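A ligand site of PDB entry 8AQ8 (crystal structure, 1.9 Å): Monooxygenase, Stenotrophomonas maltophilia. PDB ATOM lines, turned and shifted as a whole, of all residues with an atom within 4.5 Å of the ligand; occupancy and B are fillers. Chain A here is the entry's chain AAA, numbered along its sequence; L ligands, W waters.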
ATOM      1  N   ILE A  12     -31.855  -4.207  21.160  1.00  0.00           N
ATOM      2  CA  ILE A  12     -30.863  -4.405  22.263  1.00  0.00           C
ATOM      3  C   ILE A  12     -29.829  -5.395  21.726  1.00  0.00           C
ATOM      4  O   ILE A  12     -30.177  -6.555  21.490  1.00  0.00           O
ATOM      5  CB  ILE A  12     -31.539  -4.870  23.574  1.00  0.00           C
ATOM      6  CG1 ILE A  12     -32.845  -4.125  23.844  1.00  0.00           C
ATOM      7  CG2 ILE A  12     -30.584  -4.755  24.735  1.00  0.00           C
ATOM      8  CD1 ILE A  12     -32.721  -2.630  23.914  1.00  0.00           C
ATOM      9  N   GLY A  13     -28.614  -4.910  21.505  1.00  0.00           N
ATOM     10  CA  GLY A  13     -27.456  -5.712  21.072  1.00  0.00           C
ATOM     11  C   GLY A  13     -27.051  -5.421  19.652  1.00  0.00           C
ATOM     12  O   GLY A  13     -27.904  -5.488  18.749  1.00  0.00           O
ATOM     13  N   ALA A  14     -25.760  -5.176  19.452  1.00  0.00           N
ATOM     14  CA  ALA A  14     -25.150  -4.899  18.135  1.00  0.00           C
ATOM     15  C   ALA A  14     -24.291  -6.094  17.724  1.00  0.00           C
ATOM     16  O   ALA A  14     -23.186  -5.874  17.224  1.00  0.00           O
ATOM     17  CB  ALA A  14     -24.379  -3.619  18.231  1.00  0.00           C
ATOM     18  N   GLY A  15     -24.811  -7.314  17.917  1.00  0.00           N
ATOM     19  CA  GLY A  15     -24.282  -8.527  17.288  1.00  0.00           C
ATOM     20  C   GLY A  15     -24.799  -8.681  15.867  1.00  0.00           C
ATOM     21  O   GLY A  15     -25.478  -7.796  15.341  1.00  0.00           O
ATOM     22  N   PRO A  16     -24.526  -9.837  15.233  1.00  0.00           N
ATOM     23  CA  PRO A  16     -25.088 -10.126  13.917  1.00  0.00           C
ATOM     24  C   PRO A  16     -26.616 -10.009  13.863  1.00  0.00           C
ATOM     25  O   PRO A  16     -27.085  -9.452  12.907  1.00  0.00           O
ATOM     26  CB  PRO A  16     -24.626 -11.541  13.604  1.00  0.00           C
ATOM     27  CG  PRO A  16     -23.498 -11.849  14.608  1.00  0.00           C
ATOM     28  CD  PRO A  16     -23.681 -10.911  15.771  1.00  0.00           C
ATOM     29  N   ALA A  17     -27.363 -10.494  14.856  1.00  0.00           N
ATOM     30  CA  ALA A  17     -28.828 -10.400  14.866  1.00  0.00           C
ATOM     31  C   ALA A  17     -29.240  -8.928  14.906  1.00  0.00           C
ATOM     32  O   ALA A  17     -30.015  -8.499  14.040  1.00  0.00           O
ATOM     33  CB  ALA A  17     -29.428 -11.153  16.036  1.00  0.00           C
ATOM     34  N   GLY A  18     -28.772  -8.164  15.902  1.00  0.00           N
ATOM     35  CA  GLY A  18     -29.243  -6.787  16.092  1.00  0.00           C
ATOM     36  C   GLY A  18     -28.876  -5.869  14.922  1.00  0.00           C
ATOM     37  O   GLY A  18     -29.725  -5.031  14.517  1.00  0.00           O
ATOM     38  N   TYR A  35     -29.018  -0.391  20.992  1.00  0.00           N
ATOM     39  CA  TYR A  35     -28.337  -0.158  22.283  1.00  0.00           C
ATOM     40  C   TYR A  35     -27.353  -1.297  22.513  1.00  0.00           C
ATOM     41  O   TYR A  35     -27.816  -2.440  22.690  1.00  0.00           O
ATOM     42  CB  TYR A  35     -29.367   0.017  23.393  1.00  0.00           C
ATOM     43  CG  TYR A  35     -30.278   1.181  23.114  1.00  0.00           C
ATOM     44  CD1 TYR A  35     -29.937   2.466  23.492  1.00  0.00           C
ATOM     45  CD2 TYR A  35     -31.451   1.030  22.375  1.00  0.00           C
ATOM     46  CE1 TYR A  35     -30.738   3.546  23.212  1.00  0.00           C
ATOM     47  CE2 TYR A  35     -32.264   2.098  22.094  1.00  0.00           C
ATOM     48  CZ  TYR A  35     -31.912   3.365  22.518  1.00  0.00           C
ATOM     49  OH  TYR A  35     -32.694   4.464  22.263  1.00  0.00           O
ATOM     50  N   GLU A  36     -26.053  -0.979  22.521  1.00  0.00           N
ATOM     51  CA  GLU A  36     -24.948  -1.963  22.712  1.00  0.00           C
ATOM     52  C   GLU A  36     -24.217  -1.652  24.024  1.00  0.00           C
ATOM     53  O   GLU A  36     -23.678  -0.549  24.160  1.00  0.00           O
ATOM     54  CB  GLU A  36     -23.983  -1.909  21.542  1.00  0.00           C
ATOM     55  CG  GLU A  36     -22.718  -2.750  21.739  1.00  0.00           C
ATOM     56  CD  GLU A  36     -22.960  -4.213  22.058  1.00  0.00           C
ATOM     57  OE1 GLU A  36     -23.837  -4.815  21.409  1.00  0.00           O
ATOM     58  OE2 GLU A  36     -22.351  -4.708  23.041  1.00  0.00           O
ATOM     59  N   GLY A  37     -24.149  -2.637  24.921  1.00  0.00           N
ATOM     60  CA  GLY A  37     -23.422  -2.529  26.207  1.00  0.00           C
ATOM     61  C   GLY A  37     -21.968  -2.121  26.023  1.00  0.00           C
ATOM     62  O   GLY A  37     -21.506  -1.262  26.808  1.00  0.00           O
ATOM     63  N   GLU A  38     -21.270  -2.698  25.044  1.00  0.00           N
ATOM     64  CA  GLU A  38     -19.827  -2.458  24.856  1.00  0.00           C
ATOM     65  C   GLU A  38     -19.623  -1.034  24.344  1.00  0.00           C
ATOM     66  O   GLU A  38     -20.530  -0.508  23.692  1.00  0.00           O
ATOM     67  CB  GLU A  38     -19.260  -3.514  23.910  1.00  0.00           C
ATOM     68  CG  GLU A  38     -19.315  -4.922  24.483  1.00  0.00           C
ATOM     69  CD  GLU A  38     -18.795  -5.081  25.913  1.00  0.00           C
ATOM     70  OE1 GLU A  38     -19.524  -5.630  26.784  1.00  0.00           O
ATOM     71  OE2 GLU A  38     -17.633  -4.672  26.156  1.00  0.00           O
ATOM     72  N   THR A  49     -13.510 -17.403  12.567  1.00  0.00           N
ATOM     73  CA  THR A  49     -14.052 -17.498  11.188  1.00  0.00           C
ATOM     74  C   THR A  49     -15.401 -18.235  11.200  1.00  0.00           C
ATOM     75  O   THR A  49     -15.603 -19.094  12.048  1.00  0.00           O
ATOM     76  CB  THR A  49     -13.045 -18.183  10.259  1.00  0.00           C
ATOM     77  OG1 THR A  49     -11.947 -17.311  10.019  1.00  0.00           O
ATOM     78  CG2 THR A  49     -13.621 -18.551   8.914  1.00  0.00           C
ATOM     79  N   LEU A  50     -16.297 -17.895  10.257  1.00  0.00           N
ATOM     80  CA  LEU A  50     -17.596 -18.602  10.070  1.00  0.00           C
ATOM     81  C   LEU A  50     -18.020 -18.533   8.610  1.00  0.00           C
ATOM     82  O   LEU A  50     -17.489 -17.697   7.878  1.00  0.00           O
ATOM     83  CB  LEU A  50     -18.640 -17.954  10.993  1.00  0.00           C
ATOM     84  CG  LEU A  50     -18.842 -16.462  10.782  1.00  0.00           C
ATOM     85  CD1 LEU A  50     -20.075 -16.197   9.934  1.00  0.00           C
ATOM     86  CD2 LEU A  50     -18.941 -15.728  12.103  1.00  0.00           C
ATOM     87  N   ARG A 109     -15.469 -13.033  12.056  1.00  0.00           N
ATOM     88  CA  ARG A 109     -16.625 -12.522  12.835  1.00  0.00           C
ATOM     89  C   ARG A 109     -16.594 -10.996  12.871  1.00  0.00           C
ATOM     90  O   ARG A 109     -17.662 -10.389  12.726  1.00  0.00           O
ATOM     91  CB  ARG A 109     -16.616 -13.023  14.293  1.00  0.00           C
ATOM     92  CG  ARG A 109     -17.690 -12.406  15.190  1.00  0.00           C
ATOM     93  CD  ARG A 109     -17.676 -12.854  16.645  1.00  0.00           C
ATOM     94  NE  ARG A 109     -17.881 -14.303  16.632  1.00  0.00           N
ATOM     95  CZ  ARG A 109     -19.064 -14.929  16.615  1.00  0.00           C
ATOM     96  NH1 ARG A 109     -20.185 -14.222  16.687  1.00  0.00           N
ATOM     97  NH2 ARG A 109     -19.085 -16.250  16.554  1.00  0.00           N
ATOM     98  N   ARG A 113     -19.349  -8.195  11.384  1.00  0.00           N
ATOM     99  CA  ARG A 113     -19.921  -7.089  12.189  1.00  0.00           C
ATOM    100  C   ARG A 113     -19.554  -5.768  11.519  1.00  0.00           C
ATOM    101  O   ARG A 113     -20.421  -4.897  11.439  1.00  0.00           O
ATOM    102  CB  ARG A 113     -19.432  -7.123  13.638  1.00  0.00           C
ATOM    103  CG  ARG A 113     -20.492  -7.629  14.599  1.00  0.00           C
ATOM    104  CD  ARG A 113     -20.018  -7.736  16.035  1.00  0.00           C
ATOM    105  NE  ARG A 113     -20.627  -6.765  16.951  1.00  0.00           N
ATOM    106  CZ  ARG A 113     -20.004  -5.741  17.538  1.00  0.00           C
ATOM    107  NH1 ARG A 113     -18.724  -5.484  17.275  1.00  0.00           N
ATOM    108  NH2 ARG A 113     -20.669  -4.973  18.380  1.00  0.00           N
ATOM    109  N   HIS A 129     -24.437   1.484  26.221  1.00  0.00           N
ATOM    110  CA  HIS A 129     -25.826   1.358  26.703  1.00  0.00           C
ATOM    111  C   HIS A 129     -26.095  -0.117  27.006  1.00  0.00           C
ATOM    112  O   HIS A 129     -26.562  -0.843  26.125  1.00  0.00           O
ATOM    113  CB  HIS A 129     -26.796   1.967  25.695  1.00  0.00           C
ATOM    114  CG  HIS A 129     -26.758   3.459  25.652  1.00  0.00           C
ATOM    115  ND1 HIS A 129     -25.660   4.166  25.206  1.00  0.00           N
ATOM    116  CD2 HIS A 129     -27.673   4.383  26.018  1.00  0.00           C
ATOM    117  CE1 HIS A 129     -25.916   5.468  25.255  1.00  0.00           C
ATOM    118  NE2 HIS A 129     -27.150   5.615  25.720  1.00  0.00           N
ATOM    119  N   SER A 130     -25.788  -0.525  28.238  1.00  0.00           N
ATOM    120  CA  SER A 130     -26.042  -1.880  28.773  1.00  0.00           C
ATOM    121  C   SER A 130     -27.442  -1.902  29.399  1.00  0.00           C
ATOM    122  O   SER A 130     -27.629  -1.250  30.434  1.00  0.00           O
ATOM    123  CB  SER A 130     -24.943  -2.225  29.734  1.00  0.00           C
ATOM    124  OG  SER A 130     -25.161  -3.502  30.276  1.00  0.00           O
ATOM    125  N   LEU A 131     -28.402  -2.599  28.779  1.00  0.00           N
ATOM    126  CA  LEU A 131     -29.803  -2.629  29.288  1.00  0.00           C
ATOM    127  C   LEU A 131     -29.816  -3.314  30.668  1.00  0.00           C
ATOM    128  O   LEU A 131     -29.161  -4.394  30.810  1.00  0.00           O
ATOM    129  CB  LEU A 131     -30.719  -3.344  28.302  1.00  0.00           C
ATOM    130  CG  LEU A 131     -32.198  -3.274  28.661  1.00  0.00           C
ATOM    131  CD1 LEU A 131     -32.784  -1.890  28.317  1.00  0.00           C
ATOM    132  CD2 LEU A 131     -33.002  -4.374  27.975  1.00  0.00           C
ATOM    133  N   ALA A 160     -31.847  -8.724  20.956  1.00  0.00           N
ATOM    134  CA  ALA A 160     -30.753  -9.326  20.155  1.00  0.00           C
ATOM    135  C   ALA A 160     -29.511  -9.303  21.023  1.00  0.00           C
ATOM    136  O   ALA A 160     -28.423  -9.035  20.483  1.00  0.00           O
ATOM    137  CB  ALA A 160     -30.587  -8.569  18.876  1.00  0.00           C
ATOM    138  N   ASP A 161     -29.687  -9.555  22.317  1.00  0.00           N
ATOM    139  CA  ASP A 161     -28.679  -9.240  23.364  1.00  0.00           C
ATOM    140  C   ASP A 161     -28.024 -10.523  23.884  1.00  0.00           C
ATOM    141  O   ASP A 161     -27.415 -10.494  24.943  1.00  0.00           O
ATOM    142  CB  ASP A 161     -29.270  -8.319  24.436  1.00  0.00           C
ATOM    143  CG  ASP A 161     -30.597  -8.725  25.025  1.00  0.00           C
ATOM    144  OD1 ASP A 161     -31.368  -9.471  24.364  1.00  0.00           O
ATOM    145  OD2 ASP A 161     -30.865  -8.285  26.158  1.00  0.00           O
ATOM    146  N   GLY A 162     -28.099 -11.601  23.109  1.00  0.00           N
ATOM    147  CA  GLY A 162     -27.167 -12.740  23.190  1.00  0.00           C
ATOM    148  C   GLY A 162     -27.502 -13.751  24.238  1.00  0.00           C
ATOM    149  O   GLY A 162     -28.671 -13.790  24.706  1.00  0.00           O
ATOM    150  N   LYS A 166     -30.761  -9.673  28.662  1.00  0.00           N
ATOM    151  CA  LYS A 166     -31.587  -8.921  29.632  1.00  0.00           C
ATOM    152  C   LYS A 166     -33.034  -8.874  29.141  1.00  0.00           C
ATOM    153  O   LYS A 166     -33.950  -8.972  29.967  1.00  0.00           O
ATOM    154  CB  LYS A 166     -30.973  -7.530  29.852  1.00  0.00           C
ATOM    155  CG  LYS A 166     -31.478  -6.826  31.093  1.00  0.00           C
ATOM    156  CD  LYS A 166     -31.160  -7.516  32.397  1.00  0.00           C
ATOM    157  CE  LYS A 166     -29.705  -7.922  32.528  1.00  0.00           C
ATOM    158  NZ  LYS A 166     -29.371  -8.396  33.904  1.00  0.00           N
ATOM    159  N   PHE A 183     -15.095 -24.404  26.664  1.00  0.00           N
ATOM    160  CA  PHE A 183     -14.076 -24.101  25.643  1.00  0.00           C
ATOM    161  C   PHE A 183     -13.083 -23.127  26.259  1.00  0.00           C
ATOM    162  O   PHE A 183     -13.483 -22.135  26.866  1.00  0.00           O
ATOM    163  CB  PHE A 183     -14.713 -23.473  24.398  1.00  0.00           C
ATOM    164  CG  PHE A 183     -15.370 -24.413  23.426  1.00  0.00           C
ATOM    165  CD1 PHE A 183     -15.870 -25.652  23.831  1.00  0.00           C
ATOM    166  CD2 PHE A 183     -15.573 -24.021  22.114  1.00  0.00           C
ATOM    167  CE1 PHE A 183     -16.501 -26.499  22.934  1.00  0.00           C
ATOM    168  CE2 PHE A 183     -16.195 -24.877  21.222  1.00  0.00           C
ATOM    169  CZ  PHE A 183     -16.668 -26.111  21.626  1.00  0.00           C
ATOM    170  N   TYR A 226      -9.627 -23.551  20.196  1.00  0.00           N
ATOM    171  CA  TYR A 226     -10.556 -23.944  21.281  1.00  0.00           C
ATOM    172  C   TYR A 226     -10.076 -25.254  21.869  1.00  0.00           C
ATOM    173  O   TYR A 226     -10.121 -26.292  21.180  1.00  0.00           O
ATOM    174  CB  TYR A 226     -11.994 -24.057  20.765  1.00  0.00           C
ATOM    175  CG  TYR A 226     -12.599 -22.764  20.294  1.00  0.00           C
ATOM    176  CD1 TYR A 226     -12.676 -21.648  21.099  1.00  0.00           C
ATOM    177  CD2 TYR A 226     -13.173 -22.693  19.037  1.00  0.00           C
ATOM    178  CE1 TYR A 226     -13.250 -20.479  20.653  1.00  0.00           C
ATOM    179  CE2 TYR A 226     -13.739 -21.528  18.568  1.00  0.00           C
ATOM    180  CZ  TYR A 226     -13.765 -20.414  19.377  1.00  0.00           C
ATOM    181  OH  TYR A 226     -14.353 -19.290  18.886  1.00  0.00           O
ATOM    182  N   ILE A 275     -19.799 -23.500  27.959  1.00  0.00           N
ATOM    183  CA  ILE A 275     -20.815 -23.698  26.893  1.00  0.00           C
ATOM    184  C   ILE A 275     -22.164 -23.990  27.564  1.00  0.00           C
ATOM    185  O   ILE A 275     -22.356 -25.060  28.182  1.00  0.00           O
ATOM    186  CB  ILE A 275     -20.413 -24.797  25.903  1.00  0.00           C
ATOM    187  CG1 ILE A 275     -19.023 -24.564  25.305  1.00  0.00           C
ATOM    188  CG2 ILE A 275     -21.474 -24.911  24.841  1.00  0.00           C
ATOM    189  CD1 ILE A 275     -18.830 -23.200  24.673  1.00  0.00           C
ATOM    190  N   ILE A 293     -34.463 -12.625  19.298  1.00  0.00           N
ATOM    191  CA  ILE A 293     -33.841 -13.232  18.093  1.00  0.00           C
ATOM    192  C   ILE A 293     -32.432 -13.686  18.461  1.00  0.00           C
ATOM    193  O   ILE A 293     -31.868 -13.197  19.470  1.00  0.00           O
ATOM    194  CB  ILE A 293     -33.852 -12.257  16.902  1.00  0.00           C
ATOM    195  CG1 ILE A 293     -33.159 -10.936  17.227  1.00  0.00           C
ATOM    196  CG2 ILE A 293     -35.279 -12.050  16.406  1.00  0.00           C
ATOM    197  CD1 ILE A 293     -32.937 -10.053  16.036  1.00  0.00           C
ATOM    198  N   GLY A 294     -31.929 -14.620  17.673  1.00  0.00           N
ATOM    199  CA  GLY A 294     -30.581 -15.182  17.856  1.00  0.00           C
ATOM    200  C   GLY A 294     -30.461 -15.893  19.181  1.00  0.00           C
ATOM    201  O   GLY A 294     -31.416 -16.597  19.591  1.00  0.00           O
ATOM    202  N   ASP A 295     -29.299 -15.723  19.816  1.00  0.00           N
ATOM    203  CA  ASP A 295     -28.924 -16.414  21.074  1.00  0.00           C
ATOM    204  C   ASP A 295     -29.903 -16.054  22.190  1.00  0.00           C
ATOM    205  O   ASP A 295     -30.244 -16.941  22.996  1.00  0.00           O
ATOM    206  CB  ASP A 295     -27.473 -16.114  21.404  1.00  0.00           C
ATOM    207  CG  ASP A 295     -26.441 -16.955  20.651  1.00  0.00           C
ATOM    208  OD1 ASP A 295     -26.790 -17.699  19.718  1.00  0.00           O
ATOM    209  OD2 ASP A 295     -25.263 -16.843  21.036  1.00  0.00           O
ATOM    210  N   PRO A 302     -22.317 -24.735  20.254  1.00  0.00           N
ATOM    211  CA  PRO A 302     -21.715 -24.217  19.021  1.00  0.00           C
ATOM    212  C   PRO A 302     -21.489 -25.302  17.956  1.00  0.00           C
ATOM    213  O   PRO A 302     -20.363 -25.809  17.822  1.00  0.00           O
ATOM    214  CB  PRO A 302     -20.411 -23.597  19.523  1.00  0.00           C
ATOM    215  CG  PRO A 302     -20.044 -24.470  20.702  1.00  0.00           C
ATOM    216  CD  PRO A 302     -21.366 -24.827  21.359  1.00  0.00           C
ATOM    217  N   GLY A 304     -22.552 -24.919  14.713  1.00  0.00           N
ATOM    218  CA  GLY A 304     -22.341 -24.244  13.415  1.00  0.00           C
ATOM    219  C   GLY A 304     -23.627 -23.574  12.918  1.00  0.00           C
ATOM    220  O   GLY A 304     -23.690 -23.380  11.733  1.00  0.00           O
ATOM    221  N   VAL A 305     -24.577 -23.232  13.798  1.00  0.00           N
ATOM    222  CA  VAL A 305     -25.901 -22.658  13.384  1.00  0.00           C
ATOM    223  C   VAL A 305     -26.076 -21.231  13.902  1.00  0.00           C
ATOM    224  O   VAL A 305     -26.954 -20.544  13.396  1.00  0.00           O
ATOM    225  CB  VAL A 305     -27.064 -23.552  13.868  1.00  0.00           C
ATOM    226  CG1 VAL A 305     -26.933 -24.975  13.339  1.00  0.00           C
ATOM    227  CG2 VAL A 305     -27.170 -23.556  15.381  1.00  0.00           C
ATOM    228  N   GLY A 306     -25.276 -20.771  14.865  1.00  0.00           N
ATOM    229  CA  GLY A 306     -25.634 -19.612  15.706  1.00  0.00           C
ATOM    230  C   GLY A 306     -25.735 -18.299  14.949  1.00  0.00           C
ATOM    231  O   GLY A 306     -26.774 -17.606  15.065  1.00  0.00           O
ATOM    232  N   VAL A 307     -24.679 -17.913  14.210  1.00  0.00           N
ATOM    233  CA  VAL A 307     -24.666 -16.632  13.462  1.00  0.00           C
ATOM    234  C   VAL A 307     -25.717 -16.725  12.360  1.00  0.00           C
ATOM    235  O   VAL A 307     -26.440 -15.747  12.143  1.00  0.00           O
ATOM    236  CB  VAL A 307     -23.269 -16.322  12.900  1.00  0.00           C
ATOM    237  CG1 VAL A 307     -23.301 -15.110  11.997  1.00  0.00           C
ATOM    238  CG2 VAL A 307     -22.297 -16.075  14.044  1.00  0.00           C
ATOM    239  N   ASN A 308     -25.787 -17.861  11.667  1.00  0.00           N
ATOM    240  CA  ASN A 308     -26.729 -18.074  10.537  1.00  0.00           C
ATOM    241  C   ASN A 308     -28.168 -17.907  11.015  1.00  0.00           C
ATOM    242  O   ASN A 308     -28.969 -17.180  10.340  1.00  0.00           O
ATOM    243  CB  ASN A 308     -26.449 -19.385   9.806  1.00  0.00           C
ATOM    244  CG  ASN A 308     -25.319 -19.205   8.828  1.00  0.00           C
ATOM    245  OD1 ASN A 308     -25.492 -18.584   7.790  1.00  0.00           O
ATOM    246  ND2 ASN A 308     -24.137 -19.641   9.203  1.00  0.00           N
ATOM    247  N   ALA A 310     -29.157 -16.392  13.856  1.00  0.00           N
ATOM    248  CA  ALA A 310     -29.298 -15.028  14.410  1.00  0.00           C
ATOM    249  C   ALA A 310     -29.694 -14.077  13.277  1.00  0.00           C
ATOM    250  O   ALA A 310     -30.661 -13.306  13.434  1.00  0.00           O
ATOM    251  CB  ALA A 310     -28.007 -14.592  15.085  1.00  0.00           C
HETATM  252  P1  LIG L   1     -24.242 -11.929  20.078  1.00  0.00           P
HETATM  253  O1  LIG L   1     -23.359 -12.092  18.876  1.00  0.00           O
HETATM  254  O2  LIG L   1     -23.810 -12.580  21.349  1.00  0.00           O
HETATM  255  O3  LIG L   1     -24.471 -10.388  20.303  1.00  0.00           O
HETATM  256  C1  LIG L   1     -25.118  -9.959  21.489  1.00  0.00           C
HETATM  257  C2  LIG L   1     -24.787  -8.484  21.645  1.00  0.00           C
HETATM  258  O4  LIG L   1     -25.576  -7.921  22.705  1.00  0.00           O
HETATM  259  C3  LIG L   1     -23.318  -8.202  22.028  1.00  0.00           C
HETATM  260  O5  LIG L   1     -22.793  -7.192  21.201  1.00  0.00           O
HETATM  261  C4  LIG L   1     -23.394  -7.883  23.510  1.00  0.00           C
HETATM  262  O6  LIG L   1     -22.351  -7.032  23.868  1.00  0.00           O
HETATM  263  C5  LIG L   1     -24.734  -7.196  23.582  1.00  0.00           C
HETATM  264  N1  LIG L   1     -25.364  -7.185  24.893  1.00  0.00           N
HETATM  265  C6  LIG L   1     -25.446  -8.211  25.803  1.00  0.00           C
HETATM  266  N2  LIG L   1     -26.212  -7.919  26.837  1.00  0.00           N
HETATM  267  C7  LIG L   1     -26.596  -6.604  26.613  1.00  0.00           C
HETATM  268  C8  LIG L   1     -27.381  -5.705  27.365  1.00  0.00           C
HETATM  269  N3  LIG L   1     -27.952  -6.045  28.523  1.00  0.00           N
HETATM  270  N4  LIG L   1     -27.581  -4.463  26.858  1.00  0.00           N
HETATM  271  C9  LIG L   1     -26.997  -4.151  25.701  1.00  0.00           C
HETATM  272  N5  LIG L   1     -26.271  -4.936  24.895  1.00  0.00           N
HETATM  273  C10 LIG L   1     -26.097  -6.155  25.416  1.00  0.00           C
HETATM  274  N6  LIG L   1     -21.686 -19.601  15.410  1.00  0.00           N
HETATM  275  C11 LIG L   1     -21.478 -19.961  14.137  1.00  0.00           C
HETATM  276  O7  LIG L   1     -22.339 -19.798  13.272  1.00  0.00           O
HETATM  277  N7  LIG L   1     -20.314 -20.571  13.742  1.00  0.00           N
HETATM  278  C12 LIG L   1     -19.279 -20.816  14.610  1.00  0.00           C
HETATM  279  O8  LIG L   1     -18.247 -21.337  14.211  1.00  0.00           O
HETATM  280  C13 LIG L   1     -19.484 -20.505  15.967  1.00  0.00           C
HETATM  281  N8  LIG L   1     -18.530 -20.776  16.834  1.00  0.00           N
HETATM  282  C14 LIG L   1     -18.780 -20.496  18.151  1.00  0.00           C
HETATM  283  C15 LIG L   1     -17.775 -20.804  19.095  1.00  0.00           C
HETATM  284  C16 LIG L   1     -17.955 -20.548  20.440  1.00  0.00           C
HETATM  285  C17 LIG L   1     -16.862 -20.868  21.421  1.00  0.00           C
HETATM  286  C18 LIG L   1     -19.158 -19.961  20.861  1.00  0.00           C
HETATM  287  C19 LIG L   1     -19.356 -19.681  22.327  1.00  0.00           C
HETATM  288  C20 LIG L   1     -20.139 -19.624  19.951  1.00  0.00           C
HETATM  289  C21 LIG L   1     -19.979 -19.889  18.583  1.00  0.00           C
HETATM  290  N9  LIG L   1     -20.960 -19.592  17.614  1.00  0.00           N
HETATM  291  C22 LIG L   1     -20.746 -19.877  16.291  1.00  0.00           C
HETATM  292  C23 LIG L   1     -22.264 -18.975  17.952  1.00  0.00           C
HETATM  293  C24 LIG L   1     -22.304 -17.466  17.657  1.00  0.00           C
HETATM  294  O9  LIG L   1     -21.124 -16.868  18.203  1.00  0.00           O
HETATM  295  C25 LIG L   1     -23.560 -16.818  18.237  1.00  0.00           C
HETATM  296  O10 LIG L   1     -24.687 -17.672  18.070  1.00  0.00           O
HETATM  297  C26 LIG L   1     -23.949 -15.504  17.565  1.00  0.00           C
HETATM  298  O11 LIG L   1     -22.898 -14.555  17.755  1.00  0.00           O
HETATM  299  C27 LIG L   1     -25.248 -14.973  18.117  1.00  0.00           C
HETATM  300  O12 LIG L   1     -25.500 -13.647  17.564  1.00  0.00           O
HETATM  301  P2  LIG L   1     -26.469 -12.684  18.338  1.00  0.00           P
HETATM  302  O13 LIG L   1     -26.622 -11.443  17.532  1.00  0.00           O
HETATM  303  O14 LIG L   1     -27.683 -13.467  18.745  1.00  0.00           O
HETATM  304  O15 LIG L   1     -25.690 -12.471  19.715  1.00  0.00           O
HETATM  305  O   HOH W   1     -21.063 -14.375  21.045  1.00  0.00           O
HETATM  306  O   HOH W   2     -15.962 -23.893  13.647  1.00  0.00           O
HETATM  307  O   HOH W   3     -27.245  -8.884  17.995  1.00  0.00           O
HETATM  308  O   HOH W   4     -22.402 -11.377  23.233  1.00  0.00           O
HETATM  309  O   HOH W   5     -29.495 -12.490  20.529  1.00  0.00           O
HETATM  310  O   HOH W   6     -17.178 -21.639  11.557  1.00  0.00           O
HETATM  311  O   HOH W   7     -24.392 -14.698  22.549  1.00  0.00           O
HETATM  312  O   HOH W   8     -27.527  -9.051  29.172  1.00  0.00           O
HETATM  313  O   HOH W   9     -20.718 -11.172  18.413  1.00  0.00           O
HETATM  314  O   HOH W  10     -19.794  -8.519  24.205  1.00  0.00           O
HETATM  315  O   HOH W  11     -24.043  -5.556  28.490  1.00  0.00           O
HETATM  316  O   HOH W  12     -22.942 -20.827  21.224  1.00  0.00           O
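The backbone carbonyl oxygen of Leu 131 lies within hydrogen-bond range of a nitrogen (N3) of the ligand (3.1 Å).
O13 of the ligand lies within hydrogen-bond range of N of Ala 17 (2.9 Å).
N of Asp 295 is in hydrogen-bond range of O14 of the ligand.
O6 of the ligand is in hydrogen-bond range of OE2 of Glu 36 (2.5 Å).
The guanidinium group (NH2) of Arg 109 sits at hydrogen-bond distance from an oxygen (O9) of the ligand, 2.7 Å away.
N of Gly 37 is in hydrogen-bond range of N5 of the ligand.
N of Leu 131 sits at hydrogen-bond distance from N4 of the ligand (2.8 Å).
An oxygen (O7) of the ligand is in hydrogen-bond range of the backbone NH of Val 307.
The side-chain carboxylate (OD1) of Asp 295 is in hydrogen-bond range of an oxygen (O10) of the ligand (2.7 Å).
The backbone NH of Gly 306 is in hydrogen-bond range of an oxygen (O7) of the ligand (3.5 Å).
The backbone carbonyl oxygen (O) of Glu 36 lies within hydrogen-bond range of the backbone NH (N) of His 129 (3.0 Å).
N of Ala 160 lies within hydrogen-bond range of O of Ile 12, 2.8 Å away.
The side-chain carboxylate (OE1) of Glu 36 lies within hydrogen-bond range of the backbone NH (N) of Ala 14, at 2.8 Å.
O of Tyr 35 sits at hydrogen-bond distance from N of Gly 13.
N of Lys 166 is in hydrogen-bond range of OD2 of Asp 161 (2.9 Å).
The backbone carbonyl oxygen of Ala 14 is in hydrogen-bond range of the guanidinium group of Arg 113, 2.7 Å away.
N of Gly 37 lies within hydrogen-bond range of O of His 129.
The backbone NH (N) of Glu 38 lies within hydrogen-bond range of the side-chain carboxylate (OE2) of Glu 36, at 3.0 Å.
O of Asp 161 sits close to N2 of the ligand, at 3.4 Å.
CG2 of Ile 12 touches N4 of the ligand (3.7 Å).
Gly 13 touches the ligand.
Ala 14 touches the ligand.
CA of Gly 15 touches O3 of the ligand (3.5 Å).
Pro 16 touches the ligand.
O of Tyr 35 touches C9 of the ligand, at 3.6 Å.
Glu 38 touches the ligand (CG to O6, 3.7 Å).
O of His 129 touches C9 of the ligand (3.4 Å).
Ser 130 touches the ligand (CA to N4, 3.6 Å).
Ala 160 touches the ligand.
Gly 162 touches the ligand (N to C1, 3.8 Å).
Lys 166 touches the ligand (CB to N3, 3.6 Å).
Phe 183 touches the ligand.
CE1 of Tyr 226 touches C17 of the ligand, 3.7 Å away.
CA of Gly 294 touches O14 of the ligand (3.5 Å).
Pro 302 touches the ligand (CB to C14, 3.8 Å).
CB of Ala 310 touches O12 of the ligand (3.7 Å).
Hydrophobic or aromatic side chains that line the ligand: Ile 12, Pro 16, Ala 17, Leu 131, Phe 183, Tyr 226, Pro 302, Val 307 and Ala 310.
Of the 35 residues printed, 26 come within 4 Å of the ligand.
Along chain A the residues within 4 Å of the ligand span positions 12 to 310.
The nearest printed residue that does not touch the ligand is Gly 304 (4.01 Å).
Water W7 bridges O2 of the ligand (2.5 Å) and OD2 of Asp 295 (2.8 Å).
Water W3 lies within hydrogen-bond range of an oxygen (O13) of the ligand, the backbone NH (N) of Gly 18, the backbone carbonyl oxygen (O) of Ala 160 and the backbone NH (N) of Gly 15.
Water W6 lies within hydrogen-bond range of O8 of the ligand and O of Thr 49.
Water W8 bridges a nitrogen (N2) of the ligand and the backbone NH of Lys 166.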
